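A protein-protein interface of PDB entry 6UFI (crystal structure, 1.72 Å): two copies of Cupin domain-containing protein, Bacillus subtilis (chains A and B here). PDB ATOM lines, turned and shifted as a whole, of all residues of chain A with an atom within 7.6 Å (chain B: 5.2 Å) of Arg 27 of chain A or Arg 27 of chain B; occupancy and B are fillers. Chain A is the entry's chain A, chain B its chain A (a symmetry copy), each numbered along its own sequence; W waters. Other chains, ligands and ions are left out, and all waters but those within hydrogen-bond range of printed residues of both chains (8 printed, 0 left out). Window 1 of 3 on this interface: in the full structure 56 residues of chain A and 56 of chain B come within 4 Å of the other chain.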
ATOM      1  N   PRO A   8     -26.532  -4.875  27.793  1.00  0.00           N
ATOM      2  CA  PRO A   8     -26.520  -5.925  26.770  1.00  0.00           C
ATOM      3  C   PRO A   8     -25.725  -7.140  27.226  1.00  0.00           C
ATOM      4  O   PRO A   8     -24.784  -7.038  28.016  1.00  0.00           O
ATOM      5  CB  PRO A   8     -25.858  -5.245  25.569  1.00  0.00           C
ATOM      6  CG  PRO A   8     -24.953  -4.230  26.190  1.00  0.00           C
ATOM      7  CD  PRO A   8     -25.685  -3.728  27.417  1.00  0.00           C
ATOM      8  N   ARG A  23     -16.598  -5.523  33.387  1.00  0.00           N
ATOM      9  CA  ARG A  23     -16.671  -5.351  31.942  1.00  0.00           C
ATOM     10  C   ARG A  23     -16.812  -3.880  31.575  1.00  0.00           C
ATOM     11  O   ARG A  23     -17.051  -3.020  32.425  1.00  0.00           O
ATOM     12  CB  ARG A  23     -17.852  -6.142  31.367  1.00  0.00           C
ATOM     13  CG  ARG A  23     -19.175  -5.679  31.951  1.00  0.00           C
ATOM     14  CD  ARG A  23     -20.361  -6.556  31.566  1.00  0.00           C
ATOM     15  NE  ARG A  23     -20.632  -6.477  30.141  1.00  0.00           N
ATOM     16  CZ  ARG A  23     -21.803  -6.772  29.586  1.00  0.00           C
ATOM     17  NH1 ARG A  23     -22.822  -7.164  30.346  1.00  0.00           N
ATOM     18  NH2 ARG A  23     -21.953  -6.663  28.273  1.00  0.00           N
ATOM     19  N   ASN A  24     -16.690  -3.612  30.270  1.00  0.00           N
ATOM     20  CA  ASN A  24     -16.794  -2.276  29.694  1.00  0.00           C
ATOM     21  C   ASN A  24     -18.148  -2.160  28.990  1.00  0.00           C
ATOM     22  O   ASN A  24     -18.260  -2.404  27.788  1.00  0.00           O
ATOM     23  CB  ASN A  24     -15.638  -2.029  28.735  1.00  0.00           C
ATOM     24  CG  ASN A  24     -15.459  -0.569  28.414  1.00  0.00           C
ATOM     25  OD1 ASN A  24     -16.428   0.177  28.311  1.00  0.00           O
ATOM     26  ND2 ASN A  24     -14.200  -0.152  28.250  1.00  0.00           N
ATOM     27  N   ILE A  25     -19.178  -1.745  29.734  1.00  0.00           N
ATOM     28  CA  ILE A  25     -20.523  -1.734  29.159  1.00  0.00           C
ATOM     29  C   ILE A  25     -20.644  -0.661  28.084  1.00  0.00           C
ATOM     30  O   ILE A  25     -21.349  -0.850  27.087  1.00  0.00           O
ATOM     31  CB  ILE A  25     -21.579  -1.556  30.268  1.00  0.00           C
ATOM     32  CG1 ILE A  25     -21.477  -2.707  31.272  1.00  0.00           C
ATOM     33  CG2 ILE A  25     -22.985  -1.517  29.669  1.00  0.00           C
ATOM     34  CD1 ILE A  25     -22.419  -2.594  32.460  1.00  0.00           C
ATOM     35  N   GLU A  26     -19.959   0.477  28.251  1.00  0.00           N
ATOM     36  CA  GLU A  26     -20.021   1.540  27.248  1.00  0.00           C
ATOM     37  C   GLU A  26     -19.485   1.067  25.904  1.00  0.00           C
ATOM     38  O   GLU A  26     -20.075   1.345  24.853  1.00  0.00           O
ATOM     39  CB  GLU A  26     -19.236   2.767  27.717  1.00  0.00           C
ATOM     40  CG  GLU A  26     -19.814   3.472  28.931  1.00  0.00           C
ATOM     41  CD  GLU A  26     -19.394   2.849  30.255  1.00  0.00           C
ATOM     42  OE1 GLU A  26     -18.536   1.933  30.262  1.00  0.00           O
ATOM     43  OE2 GLU A  26     -19.936   3.279  31.295  1.00  0.00           O
ATOM     44  N   ARG A  27     -18.367   0.340  25.910  1.00  0.00           N
ATOM     45  CA  ARG A  27     -17.849  -0.184  24.651  1.00  0.00           C
ATOM     46  C   ARG A  27     -18.744  -1.289  24.103  1.00  0.00           C
ATOM     47  O   ARG A  27     -18.955  -1.375  22.891  1.00  0.00           O
ATOM     48  CB  ARG A  27     -16.405  -0.672  24.829  1.00  0.00           C
ATOM     49  CG  ARG A  27     -15.405   0.458  24.754  1.00  0.00           C
ATOM     50  CD  ARG A  27     -13.946   0.013  24.897  1.00  0.00           C
ATOM     51  NE  ARG A  27     -13.105   1.159  25.271  1.00  0.00           N
ATOM     52  CZ  ARG A  27     -12.032   1.582  24.601  1.00  0.00           C
ATOM     53  NH1 ARG A  27     -11.604   0.944  23.518  1.00  0.00           N
ATOM     54  NH2 ARG A  27     -11.370   2.639  25.041  1.00  0.00           N
ATOM     55  N   ASP A  28     -19.306  -2.133  24.977  1.00  0.00           N
ATOM     56  CA  ASP A  28     -20.220  -3.166  24.495  1.00  0.00           C
ATOM     57  C   ASP A  28     -21.419  -2.544  23.783  1.00  0.00           C
ATOM     58  O   ASP A  28     -21.878  -3.062  22.761  1.00  0.00           O
ATOM     59  CB  ASP A  28     -20.703  -4.056  25.649  1.00  0.00           C
ATOM     60  CG  ASP A  28     -19.620  -4.995  26.175  1.00  0.00           C
ATOM     61  OD1 ASP A  28     -18.595  -5.200  25.486  1.00  0.00           O
ATOM     62  OD2 ASP A  28     -19.795  -5.540  27.287  1.00  0.00           O
ATOM     63  N   ARG A  29     -21.930  -1.421  24.305  1.00  0.00           N
ATOM     64  CA  ARG A  29     -23.060  -0.765  23.657  1.00  0.00           C
ATOM     65  C   ARG A  29     -22.681  -0.211  22.290  1.00  0.00           C
ATOM     66  O   ARG A  29     -23.543  -0.124  21.407  1.00  0.00           O
ATOM     67  CB  ARG A  29     -23.619   0.352  24.547  1.00  0.00           C
ATOM     68  CG  ARG A  29     -24.345  -0.127  25.799  1.00  0.00           C
ATOM     69  CD  ARG A  29     -25.016   1.061  26.503  1.00  0.00           C
ATOM     70  NE  ARG A  29     -25.494   0.741  27.850  1.00  0.00           N
ATOM     71  CZ  ARG A  29     -25.062   1.321  28.972  1.00  0.00           C
ATOM     72  NH1 ARG A  29     -24.135   2.274  28.942  1.00  0.00           N
ATOM     73  NH2 ARG A  29     -25.572   0.948  30.140  1.00  0.00           N
ATOM     74  N   GLN A  30     -21.412   0.161  22.093  1.00  0.00           N
ATOM     75  CA  GLN A  30     -20.964   0.653  20.796  1.00  0.00           C
ATOM     76  C   GLN A  30     -20.746  -0.468  19.790  1.00  0.00           C
ATOM     77  O   GLN A  30     -20.733  -0.197  18.582  1.00  0.00           O
ATOM     78  CB  GLN A  30     -19.670   1.463  20.934  1.00  0.00           C
ATOM     79  CG  GLN A  30     -19.855   2.731  21.772  1.00  0.00           C
ATOM     80  CD  GLN A  30     -18.671   3.681  21.700  1.00  0.00           C
ATOM     81  OE1 GLN A  30     -17.607   3.335  21.198  1.00  0.00           O
ATOM     82  NE2 GLN A  30     -18.863   4.899  22.207  1.00  0.00           N
ATOM     83  N   ASN A  31     -20.607  -1.711  20.258  1.00  0.00           N
ATOM     84  CA  ASN A  31     -20.229  -2.854  19.430  1.00  0.00           C
ATOM     85  C   ASN A  31     -21.265  -3.975  19.478  1.00  0.00           C
ATOM     86  O   ASN A  31     -20.927  -5.127  19.785  1.00  0.00           O
ATOM     87  CB  ASN A  31     -18.874  -3.386  19.888  1.00  0.00           C
ATOM     88  CG  ASN A  31     -17.762  -2.394  19.675  1.00  0.00           C
ATOM     89  OD1 ASN A  31     -17.841  -1.552  18.781  1.00  0.00           O
ATOM     90  ND2 ASN A  31     -16.707  -2.495  20.480  1.00  0.00           N
ATOM     91  N   PRO A  32     -22.531  -3.691  19.167  1.00  0.00           N
ATOM     92  CA  PRO A  32     -23.555  -4.732  19.360  1.00  0.00           C
ATOM     93  C   PRO A  32     -23.346  -5.956  18.485  1.00  0.00           C
ATOM     94  O   PRO A  32     -23.711  -7.071  18.893  1.00  0.00           O
ATOM     95  CB  PRO A  32     -24.862  -4.004  19.012  1.00  0.00           C
ATOM     96  CG  PRO A  32     -24.434  -2.909  18.066  1.00  0.00           C
ATOM     97  CD  PRO A  32     -23.108  -2.455  18.607  1.00  0.00           C
ATOM     98  N   MET A  34     -20.504  -7.171  17.623  1.00  0.00           N
ATOM     99  CA  MET A  34     -19.345  -7.905  18.089  1.00  0.00           C
ATOM    100  C   MET A  34     -19.625  -8.639  19.396  1.00  0.00           C
ATOM    101  O   MET A  34     -19.230  -9.801  19.524  1.00  0.00           O
ATOM    102  CB  MET A  34     -18.162  -6.940  18.202  1.00  0.00           C
ATOM    103  CG  MET A  34     -17.994  -6.189  16.870  1.00  0.00           C
ATOM    104  SD  MET A  34     -16.787  -4.860  16.841  1.00  0.00           S
ATOM    105  CE  MET A  34     -15.290  -5.817  16.982  1.00  0.00           C
ATOM    106  N   LEU A  35     -20.352  -8.021  20.337  1.00  0.00           N
ATOM    107  CA  LEU A  35     -20.829  -8.767  21.503  1.00  0.00           C
ATOM    108  C   LEU A  35     -21.779  -9.889  21.089  1.00  0.00           C
ATOM    109  O   LEU A  35     -21.732 -10.993  21.654  1.00  0.00           O
ATOM    110  CB  LEU A  35     -21.526  -7.819  22.477  1.00  0.00           C
ATOM    111  CG  LEU A  35     -21.891  -8.424  23.835  1.00  0.00           C
ATOM    112  CD1 LEU A  35     -20.650  -8.636  24.678  1.00  0.00           C
ATOM    113  CD2 LEU A  35     -22.898  -7.511  24.555  1.00  0.00           C
ATOM    114  N   LYS A  49     -10.784  -2.642  12.762  1.00  0.00           N
ATOM    115  CA  LYS A  49     -11.428  -1.475  13.355  1.00  0.00           C
ATOM    116  C   LYS A  49     -10.523  -0.851  14.413  1.00  0.00           C
ATOM    117  O   LYS A  49      -9.989  -1.564  15.263  1.00  0.00           O
ATOM    118  CB  LYS A  49     -12.778  -1.910  13.948  1.00  0.00           C
ATOM    119  CG  LYS A  49     -13.274  -1.177  15.162  1.00  0.00           C
ATOM    120  CD  LYS A  49     -14.385  -2.013  15.800  1.00  0.00           C
ATOM    121  CE  LYS A  49     -14.934  -1.389  17.069  1.00  0.00           C
ATOM    122  NZ  LYS A  49     -15.878  -0.301  16.768  1.00  0.00           N
ATOM    123  N   PHE A  50     -10.356   0.478  14.370  1.00  0.00           N
ATOM    124  CA  PHE A  50      -9.606   1.175  15.415  1.00  0.00           C
ATOM    125  C   PHE A  50     -10.123   2.607  15.538  1.00  0.00           C
ATOM    126  O   PHE A  50     -10.373   3.265  14.525  1.00  0.00           O
ATOM    127  CB  PHE A  50      -8.088   1.192  15.144  1.00  0.00           C
ATOM    128  CG  PHE A  50      -7.262   1.345  16.398  1.00  0.00           C
ATOM    129  CD1 PHE A  50      -6.913   2.608  16.882  1.00  0.00           C
ATOM    130  CD2 PHE A  50      -6.880   0.221  17.123  1.00  0.00           C
ATOM    131  CE1 PHE A  50      -6.193   2.736  18.062  1.00  0.00           C
ATOM    132  CE2 PHE A  50      -6.135   0.341  18.290  1.00  0.00           C
ATOM    133  CZ  PHE A  50      -5.783   1.603  18.756  1.00  0.00           C
ATOM    134  N   SER A  51     -10.230   3.111  16.776  1.00  0.00           N
ATOM    135  CA  SER A  51     -10.767   4.443  17.033  1.00  0.00           C
ATOM    136  C   SER A  51      -9.651   5.454  17.272  1.00  0.00           C
ATOM    137  O   SER A  51      -8.723   5.195  18.045  1.00  0.00           O
ATOM    138  CB  SER A  51     -11.692   4.435  18.248  1.00  0.00           C
ATOM    139  OG  SER A  51     -12.164   5.750  18.504  1.00  0.00           O
ATOM    140  N   PHE A  52      -9.761   6.629  16.629  1.00  0.00           N
ATOM    141  CA  PHE A  52      -8.841   7.720  16.963  1.00  0.00           C
ATOM    142  C   PHE A  52      -8.927   8.094  18.442  1.00  0.00           C
ATOM    143  O   PHE A  52      -7.950   8.599  19.009  1.00  0.00           O
ATOM    144  CB  PHE A  52      -9.125   8.969  16.109  1.00  0.00           C
ATOM    145  CG  PHE A  52      -8.400   8.987  14.773  1.00  0.00           C
ATOM    146  CD1 PHE A  52      -7.056   9.344  14.691  1.00  0.00           C
ATOM    147  CD2 PHE A  52      -9.070   8.661  13.605  1.00  0.00           C
ATOM    148  CE1 PHE A  52      -6.401   9.372  13.478  1.00  0.00           C
ATOM    149  CE2 PHE A  52      -8.414   8.682  12.383  1.00  0.00           C
ATOM    150  CZ  PHE A  52      -7.072   9.051  12.322  1.00  0.00           C
ATOM    151  N   SER A  53     -10.086   7.872  19.086  1.00  0.00           N
ATOM    152  CA  SER A  53     -10.192   8.190  20.505  1.00  0.00           C
ATOM    153  C   SER A  53      -9.310   7.303  21.372  1.00  0.00           C
ATOM    154  O   SER A  53      -9.062   7.645  22.540  1.00  0.00           O
ATOM    155  CB  SER A  53     -11.646   8.081  20.959  1.00  0.00           C
ATOM    156  OG  SER A  53     -12.373   9.197  20.497  1.00  0.00           O
ATOM    157  N   ASP A  54      -8.821   6.186  20.834  1.00  0.00           N
ATOM    158  CA  ASP A  54      -7.914   5.306  21.542  1.00  0.00           C
ATOM    159  C   ASP A  54      -6.443   5.611  21.232  1.00  0.00           C
ATOM    160  O   ASP A  54      -5.578   4.746  21.433  1.00  0.00           O
ATOM    161  CB  ASP A  54      -8.259   3.850  21.209  1.00  0.00           C
ATOM    162  CG  ASP A  54      -9.562   3.391  21.871  1.00  0.00           C
ATOM    163  OD1 ASP A  54      -9.811   3.766  23.030  1.00  0.00           O
ATOM    164  OD2 ASP A  54     -10.348   2.650  21.236  1.00  0.00           O
ATOM    165  N   ASN A 304     -18.417  -3.189  13.986  1.00  0.00           N
ATOM    166  CA  ASN A 304     -19.182  -1.956  14.163  1.00  0.00           C
ATOM    167  C   ASN A 304     -18.270  -0.745  14.046  1.00  0.00           C
ATOM    168  O   ASN A 304     -17.124  -0.776  14.496  1.00  0.00           O
ATOM    169  CB  ASN A 304     -19.851  -1.914  15.535  1.00  0.00           C
ATOM    170  CG  ASN A 304     -20.991  -2.882  15.643  1.00  0.00           C
ATOM    171  OD1 ASN A 304     -20.908  -3.860  16.377  1.00  0.00           O
ATOM    172  ND2 ASN A 304     -22.063  -2.625  14.904  1.00  0.00           N
ATOM    173  N   GLN A 306     -18.300   3.865  14.130  1.00  0.00           N
ATOM    174  CA  GLN A 306     -18.974   5.151  14.290  1.00  0.00           C
ATOM    175  C   GLN A 306     -17.953   6.261  14.099  1.00  0.00           C
ATOM    176  O   GLN A 306     -16.774   6.003  13.849  1.00  0.00           O
ATOM    177  CB  GLN A 306     -19.693   5.241  15.641  1.00  0.00           C
ATOM    178  CG  GLN A 306     -18.818   5.127  16.873  1.00  0.00           C
ATOM    179  CD  GLN A 306     -19.673   5.085  18.134  1.00  0.00           C
ATOM    180  OE1 GLN A 306     -20.298   4.062  18.445  1.00  0.00           O
ATOM    181  NE2 GLN A 306     -19.752   6.207  18.834  1.00  0.00           N
ATOM    182  N   ALA A 307     -18.427   7.510  14.201  1.00  0.00           N
ATOM    183  CA  ALA A 307     -17.575   8.673  13.958  1.00  0.00           C
ATOM    184  C   ALA A 307     -16.254   8.540  14.699  1.00  0.00           C
ATOM    185  O   ALA A 307     -16.228   8.212  15.890  1.00  0.00           O
ATOM    186  CB  ALA A 307     -18.297   9.957  14.399  1.00  0.00           C
ATOM    187  N   ASP A 309     -13.805   6.365  13.762  1.00  0.00           N
ATOM    188  CA  ASP A 309     -13.220   5.039  13.592  1.00  0.00           C
ATOM    189  C   ASP A 309     -12.536   4.908  12.241  1.00  0.00           C
ATOM    190  O   ASP A 309     -12.990   5.454  11.232  1.00  0.00           O
ATOM    191  CB  ASP A 309     -14.283   3.939  13.701  1.00  0.00           C
ATOM    192  CG  ASP A 309     -14.730   3.701  15.122  1.00  0.00           C
ATOM    193  OD1 ASP A 309     -14.010   4.130  16.044  1.00  0.00           O
ATOM    194  OD2 ASP A 309     -15.794   3.066  15.313  1.00  0.00           O
ATOM    195  N   ASN B  24     -16.119  10.499  19.318  1.00  0.00           N
ATOM    196  CA  ASN B  24     -16.548   9.449  20.237  1.00  0.00           C
ATOM    197  C   ASN B  24     -16.328   9.944  21.668  1.00  0.00           C
ATOM    198  O   ASN B  24     -15.288   9.688  22.275  1.00  0.00           O
ATOM    199  CB  ASN B  24     -15.778   8.166  19.960  1.00  0.00           C
ATOM    200  CG  ASN B  24     -16.427   6.959  20.584  1.00  0.00           C
ATOM    201  OD1 ASN B  24     -16.993   7.039  21.671  1.00  0.00           O
ATOM    202  ND2 ASN B  24     -16.347   5.821  19.889  1.00  0.00           N
ATOM    203  N   ILE B  25     -17.333  10.624  22.229  1.00  0.00           N
ATOM    204  CA  ILE B  25     -17.144  11.234  23.545  1.00  0.00           C
ATOM    205  C   ILE B  25     -17.034  10.168  24.627  1.00  0.00           C
ATOM    206  O   ILE B  25     -16.286  10.334  25.596  1.00  0.00           O
ATOM    207  CB  ILE B  25     -18.278  12.236  23.840  1.00  0.00           C
ATOM    208  CG1 ILE B  25     -18.289  13.338  22.778  1.00  0.00           C
ATOM    209  CG2 ILE B  25     -18.099  12.858  25.226  1.00  0.00           C
ATOM    210  CD1 ILE B  25     -19.422  14.341  22.920  1.00  0.00           C
ATOM    211  N   GLU B  26     -17.759   9.050  24.485  1.00  0.00           N
ATOM    212  CA  GLU B  26     -17.686   7.982  25.481  1.00  0.00           C
ATOM    213  C   GLU B  26     -16.280   7.410  25.580  1.00  0.00           C
ATOM    214  O   GLU B  26     -15.767   7.174  26.681  1.00  0.00           O
ATOM    215  CB  GLU B  26     -18.679   6.867  25.146  1.00  0.00           C
ATOM    216  CG  GLU B  26     -20.142   7.261  25.240  1.00  0.00           C
ATOM    217  CD  GLU B  26     -20.672   7.943  23.987  1.00  0.00           C
ATOM    218  OE1 GLU B  26     -19.947   8.007  22.965  1.00  0.00           O
ATOM    219  OE2 GLU B  26     -21.824   8.424  24.033  1.00  0.00           O
ATOM    220  N   ARG B  27     -15.626   7.184  24.439  1.00  0.00           N
ATOM    221  CA  ARG B  27     -14.255   6.691  24.486  1.00  0.00           C
ATOM    222  C   ARG B  27     -13.300   7.764  24.995  1.00  0.00           C
ATOM    223  O   ARG B  27     -12.369   7.462  25.746  1.00  0.00           O
ATOM    224  CB  ARG B  27     -13.827   6.171  23.107  1.00  0.00           C
ATOM    225  CG  ARG B  27     -14.309   4.763  22.851  1.00  0.00           C
ATOM    226  CD  ARG B  27     -13.878   4.190  21.496  1.00  0.00           C
ATOM    227  NE  ARG B  27     -14.737   3.055  21.134  1.00  0.00           N
ATOM    228  CZ  ARG B  27     -14.311   1.825  20.842  1.00  0.00           C
ATOM    229  NH1 ARG B  27     -13.015   1.535  20.820  1.00  0.00           N
ATOM    230  NH2 ARG B  27     -15.195   0.887  20.545  1.00  0.00           N
ATOM    231  N   ASP B  28     -13.524   9.030  24.626  1.00  0.00           N
ATOM    232  CA  ASP B  28     -12.668  10.095  25.144  1.00  0.00           C
ATOM    233  C   ASP B  28     -12.735  10.154  26.668  1.00  0.00           C
ATOM    234  O   ASP B  28     -11.717  10.372  27.333  1.00  0.00           O
ATOM    235  CB  ASP B  28     -13.060  11.455  24.551  1.00  0.00           C
ATOM    236  CG  ASP B  28     -12.671  11.603  23.082  1.00  0.00           C
ATOM    237  OD1 ASP B  28     -11.841  10.810  22.582  1.00  0.00           O
ATOM    238  OD2 ASP B  28     -13.195  12.524  22.418  1.00  0.00           O
ATOM    239  N   ARG B  29     -13.930   9.949  27.240  1.00  0.00           N
ATOM    240  CA  ARG B  29     -14.055   9.969  28.692  1.00  0.00           C
ATOM    241  C   ARG B  29     -13.308   8.809  29.338  1.00  0.00           C
ATOM    242  O   ARG B  29     -12.848   8.938  30.479  1.00  0.00           O
ATOM    243  CB  ARG B  29     -15.531   9.947  29.108  1.00  0.00           C
ATOM    244  CG  ARG B  29     -16.300  11.230  28.814  1.00  0.00           C
ATOM    245  CD  ARG B  29     -17.701  11.157  29.438  1.00  0.00           C
ATOM    246  NE  ARG B  29     -18.598  12.218  28.974  1.00  0.00           N
ATOM    247  CZ  ARG B  29     -19.735  12.017  28.303  1.00  0.00           C
ATOM    248  NH1 ARG B  29     -20.152  10.790  28.006  1.00  0.00           N
ATOM    249  NH2 ARG B  29     -20.469  13.059  27.933  1.00  0.00           N
ATOM    250  N   GLN B  30     -13.172   7.680  28.633  1.00  0.00           N
ATOM    251  CA  GLN B  30     -12.426   6.546  29.166  1.00  0.00           C
ATOM    252  C   GLN B  30     -10.919   6.739  29.066  1.00  0.00           C
ATOM    253  O   GLN B  30     -10.179   6.062  29.790  1.00  0.00           O
ATOM    254  CB  GLN B  30     -12.815   5.249  28.447  1.00  0.00           C
ATOM    255  CG  GLN B  30     -14.282   4.871  28.669  1.00  0.00           C
ATOM    256  CD  GLN B  30     -14.620   3.465  28.198  1.00  0.00           C
ATOM    257  OE1 GLN B  30     -13.836   2.816  27.515  1.00  0.00           O
ATOM    258  NE2 GLN B  30     -15.808   2.990  28.576  1.00  0.00           N
ATOM    259  N   ASN B  31     -10.462   7.661  28.215  1.00  0.00           N
ATOM    260  CA  ASN B  31      -9.048   7.840  27.895  1.00  0.00           C
ATOM    261  C   ASN B  31      -8.557   9.254  28.195  1.00  0.00           C
ATOM    262  O   ASN B  31      -7.999   9.924  27.315  1.00  0.00           O
ATOM    263  CB  ASN B  31      -8.817   7.518  26.420  1.00  0.00           C
ATOM    264  CG  ASN B  31      -9.089   6.075  26.094  1.00  0.00           C
ATOM    265  OD1 ASN B  31      -8.962   5.207  26.958  1.00  0.00           O
ATOM    266  ND2 ASN B  31      -9.447   5.800  24.842  1.00  0.00           N
ATOM    267  N   LYS B  49      -2.492  -0.983  24.303  1.00  0.00           N
ATOM    268  CA  LYS B  49      -3.790  -1.104  24.956  1.00  0.00           C
ATOM    269  C   LYS B  49      -4.824  -1.660  23.980  1.00  0.00           C
ATOM    270  O   LYS B  49      -4.920  -1.183  22.849  1.00  0.00           O
ATOM    271  CB  LYS B  49      -4.200   0.276  25.491  1.00  0.00           C
ATOM    272  CG  LYS B  49      -5.666   0.600  25.535  1.00  0.00           C
ATOM    273  CD  LYS B  49      -5.813   2.113  25.704  1.00  0.00           C
ATOM    274  CE  LYS B  49      -7.262   2.564  25.716  1.00  0.00           C
ATOM    275  NZ  LYS B  49      -7.890   2.322  27.025  1.00  0.00           N
ATOM    276  N   SER B  51      -9.062  -3.499  24.145  1.00  0.00           N
ATOM    277  CA  SER B  51     -10.193  -3.933  24.959  1.00  0.00           C
ATOM    278  C   SER B  51     -10.816  -5.209  24.405  1.00  0.00           C
ATOM    279  O   SER B  51     -11.071  -5.312  23.200  1.00  0.00           O
ATOM    280  CB  SER B  51     -11.267  -2.850  25.025  1.00  0.00           C
ATOM    281  OG  SER B  51     -12.375  -3.314  25.783  1.00  0.00           O
ATOM    282  N   SER B  53     -13.791  -5.793  24.776  1.00  0.00           N
ATOM    283  CA  SER B  53     -15.080  -5.359  24.252  1.00  0.00           C
ATOM    284  C   SER B  53     -15.018  -4.981  22.779  1.00  0.00           C
ATOM    285  O   SER B  53     -16.071  -4.889  22.128  1.00  0.00           O
ATOM    286  CB  SER B  53     -15.610  -4.182  25.070  1.00  0.00           C
ATOM    287  OG  SER B  53     -16.096  -4.646  26.309  1.00  0.00           O
ATOM    288  N   ASP B  54     -13.819  -4.772  22.235  1.00  0.00           N
ATOM    289  CA  ASP B  54     -13.637  -4.478  20.828  1.00  0.00           C
ATOM    290  C   ASP B  54     -13.337  -5.736  20.003  1.00  0.00           C
ATOM    291  O   ASP B  54     -12.789  -5.631  18.897  1.00  0.00           O
ATOM    292  CB  ASP B  54     -12.525  -3.435  20.670  1.00  0.00           C
ATOM    293  CG  ASP B  54     -12.963  -2.039  21.124  1.00  0.00           C
ATOM    294  OD1 ASP B  54     -14.118  -1.658  20.866  1.00  0.00           O
ATOM    295  OD2 ASP B  54     -12.154  -1.310  21.744  1.00  0.00           O
HETATM  296  O   HOH W   1     -15.487  -5.723  28.749  1.00  0.00           O
HETATM  297  O   HOH W   2     -13.424  10.512  18.341  1.00  0.00           O
HETATM  298  O   HOH W   3      -9.238  10.305  23.318  1.00  0.00           O
HETATM  299  O   HOH W   4     -14.823   6.331  17.316  1.00  0.00           O
HETATM  300  O   HOH W   5     -12.315  -2.497  28.637  1.00  0.00           O
HETATM  301  O   HOH W   6     -11.759  -3.232  17.274  1.00  0.00           O
HETATM  302  O   HOH W   7     -18.373  -6.216  22.938  1.00  0.00           O
HETATM  303  O   HOH W   8      -5.692   1.854  22.468  1.00  0.00           O
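The side-chain carboxylate (OE1) of Glu 26 of chain A lies within hydrogen-bond range of the side-chain amide nitrogen (NE2) of Gln 30 of chain B (3.4 Å).
The guanidinium group of Arg 27 of chain A sits close to the guanidinium group of Arg 27 of chain B (3.1 Å).
The side-chain amide nitrogen of Gln 30 of chain A lies within hydrogen-bond range of the side-chain amide oxygen of Asn 24 of chain B (2.9 Å).
NE of Arg 27 of chain A lies within hydrogen-bond range of OE1 of Gln 30 of chain B, at 2.9 Å.
The guanidinium group of Arg 27 of chain B lies within salt-bridge range of the side-chain carboxylate of Asp 54 of chain A (2.9 Å).
The backbone carbonyl oxygen (O) of Ser 53 of chain B sits at hydrogen-bond distance from the side-chain amide nitrogen (ND2) of Asn 31 of chain A, at 3.0 Å.
O of Ser 53 of chain A sits at hydrogen-bond distance from ND2 of Asn 31 of chain B (3.0 Å).
OD1 of Asp 28 of chain A lies within hydrogen-bond range of OG of Ser 53 of chain B.
The side-chain carboxylate (OD1) of Asp 28 of chain B is in hydrogen-bond range of the side-chain hydroxyl (OG) of Ser 53 of chain A (2.7 Å).
OE1 of Gln 30 of chain A sits at hydrogen-bond distance from NE of Arg 27 of chain B (2.9 Å).
The side-chain amide oxygen (OD1) of Asn 24 of chain A is in hydrogen-bond range of the side-chain amide nitrogen (NE2) of Gln 30 of chain B (2.9 Å).
The side-chain carboxylate (OD1) of Asp 54 of chain A is in hydrogen-bond range of the side-chain amide nitrogen (ND2) of Asn 31 of chain B (2.7 Å).
The side-chain carboxylate (OD2) of Asp 54 of chain B is in salt-bridge range of the guanidinium group (NH1) of Arg 27 of chain A, at 2.9 Å.
ND2 of Asn 31 of chain A lies within hydrogen-bond range of OD1 of Asp 54 of chain B (2.7 Å).
The side-chain hydroxyl of Ser 53 of chain A lies within hydrogen-bond range of the backbone carbonyl oxygen of Asn 24 of chain B (3.4 Å).
The side-chain carboxylate (OE1) of Glu 26 of chain B sits at hydrogen-bond distance from the side-chain amide nitrogen (NE2) of Gln 30 of chain A, 3.4 Å away.
The side-chain hydroxyl (OG) of Ser 51 of chain A sits close to the side-chain carboxylate (OD1) of Asp 309 of chain A (3.5 Å).
Pro 8 of chain A touches none of the printed residues of chain B.
Printed residues of chain A within 4 Å of Asp 54 of chain B: Arg 27 (2.9 Å), Asn 31 (2.7 Å), Met 34 (3.2 Å) and Lys 49 (3.9 Å).
The nearest printed residue of chain B that does not touch Arg 27 of chain A is Lys 49 of chain B (4.02 Å).
Of the 12 printed residues of chain B, 10 touch a printed residue of chain A.
Printed residues of chain B that touch a printed residue of chain A: Asn 24, Glu 26, Arg 27, Asp 28, Gln 30, Asn 31, Lys 49, Ser 51, Ser 53 and Asp 54.
Hydrophobic or aromatic side chains of chain A within 4 Å of the printed part of chain B: Met 34.
Among the printed residues, Asp or Glu carboxylates within 4 Å of a Lys or Arg side-chain nitrogen of the other chain: Arg 27 of chain A with Asp 54 of chain B (2.9 Å) and Asp 54 of chain A with Arg 27 of chain B (2.9 Å).
Arg 27 of chain A touches Ser 51 of chain B, and with the chains exchanged Ser 51 of chain A touches Arg 27 of chain B.
Asn 31 of chain A touches Asp 54 of chain B, and with the chains exchanged Asp 54 of chain A touches Asn 31 of chain B.
Water W8 bridges the backbone carbonyl oxygen (O) of Asp 54 of chain A and the backbone carbonyl oxygen (O) of Lys 49 of chain B.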
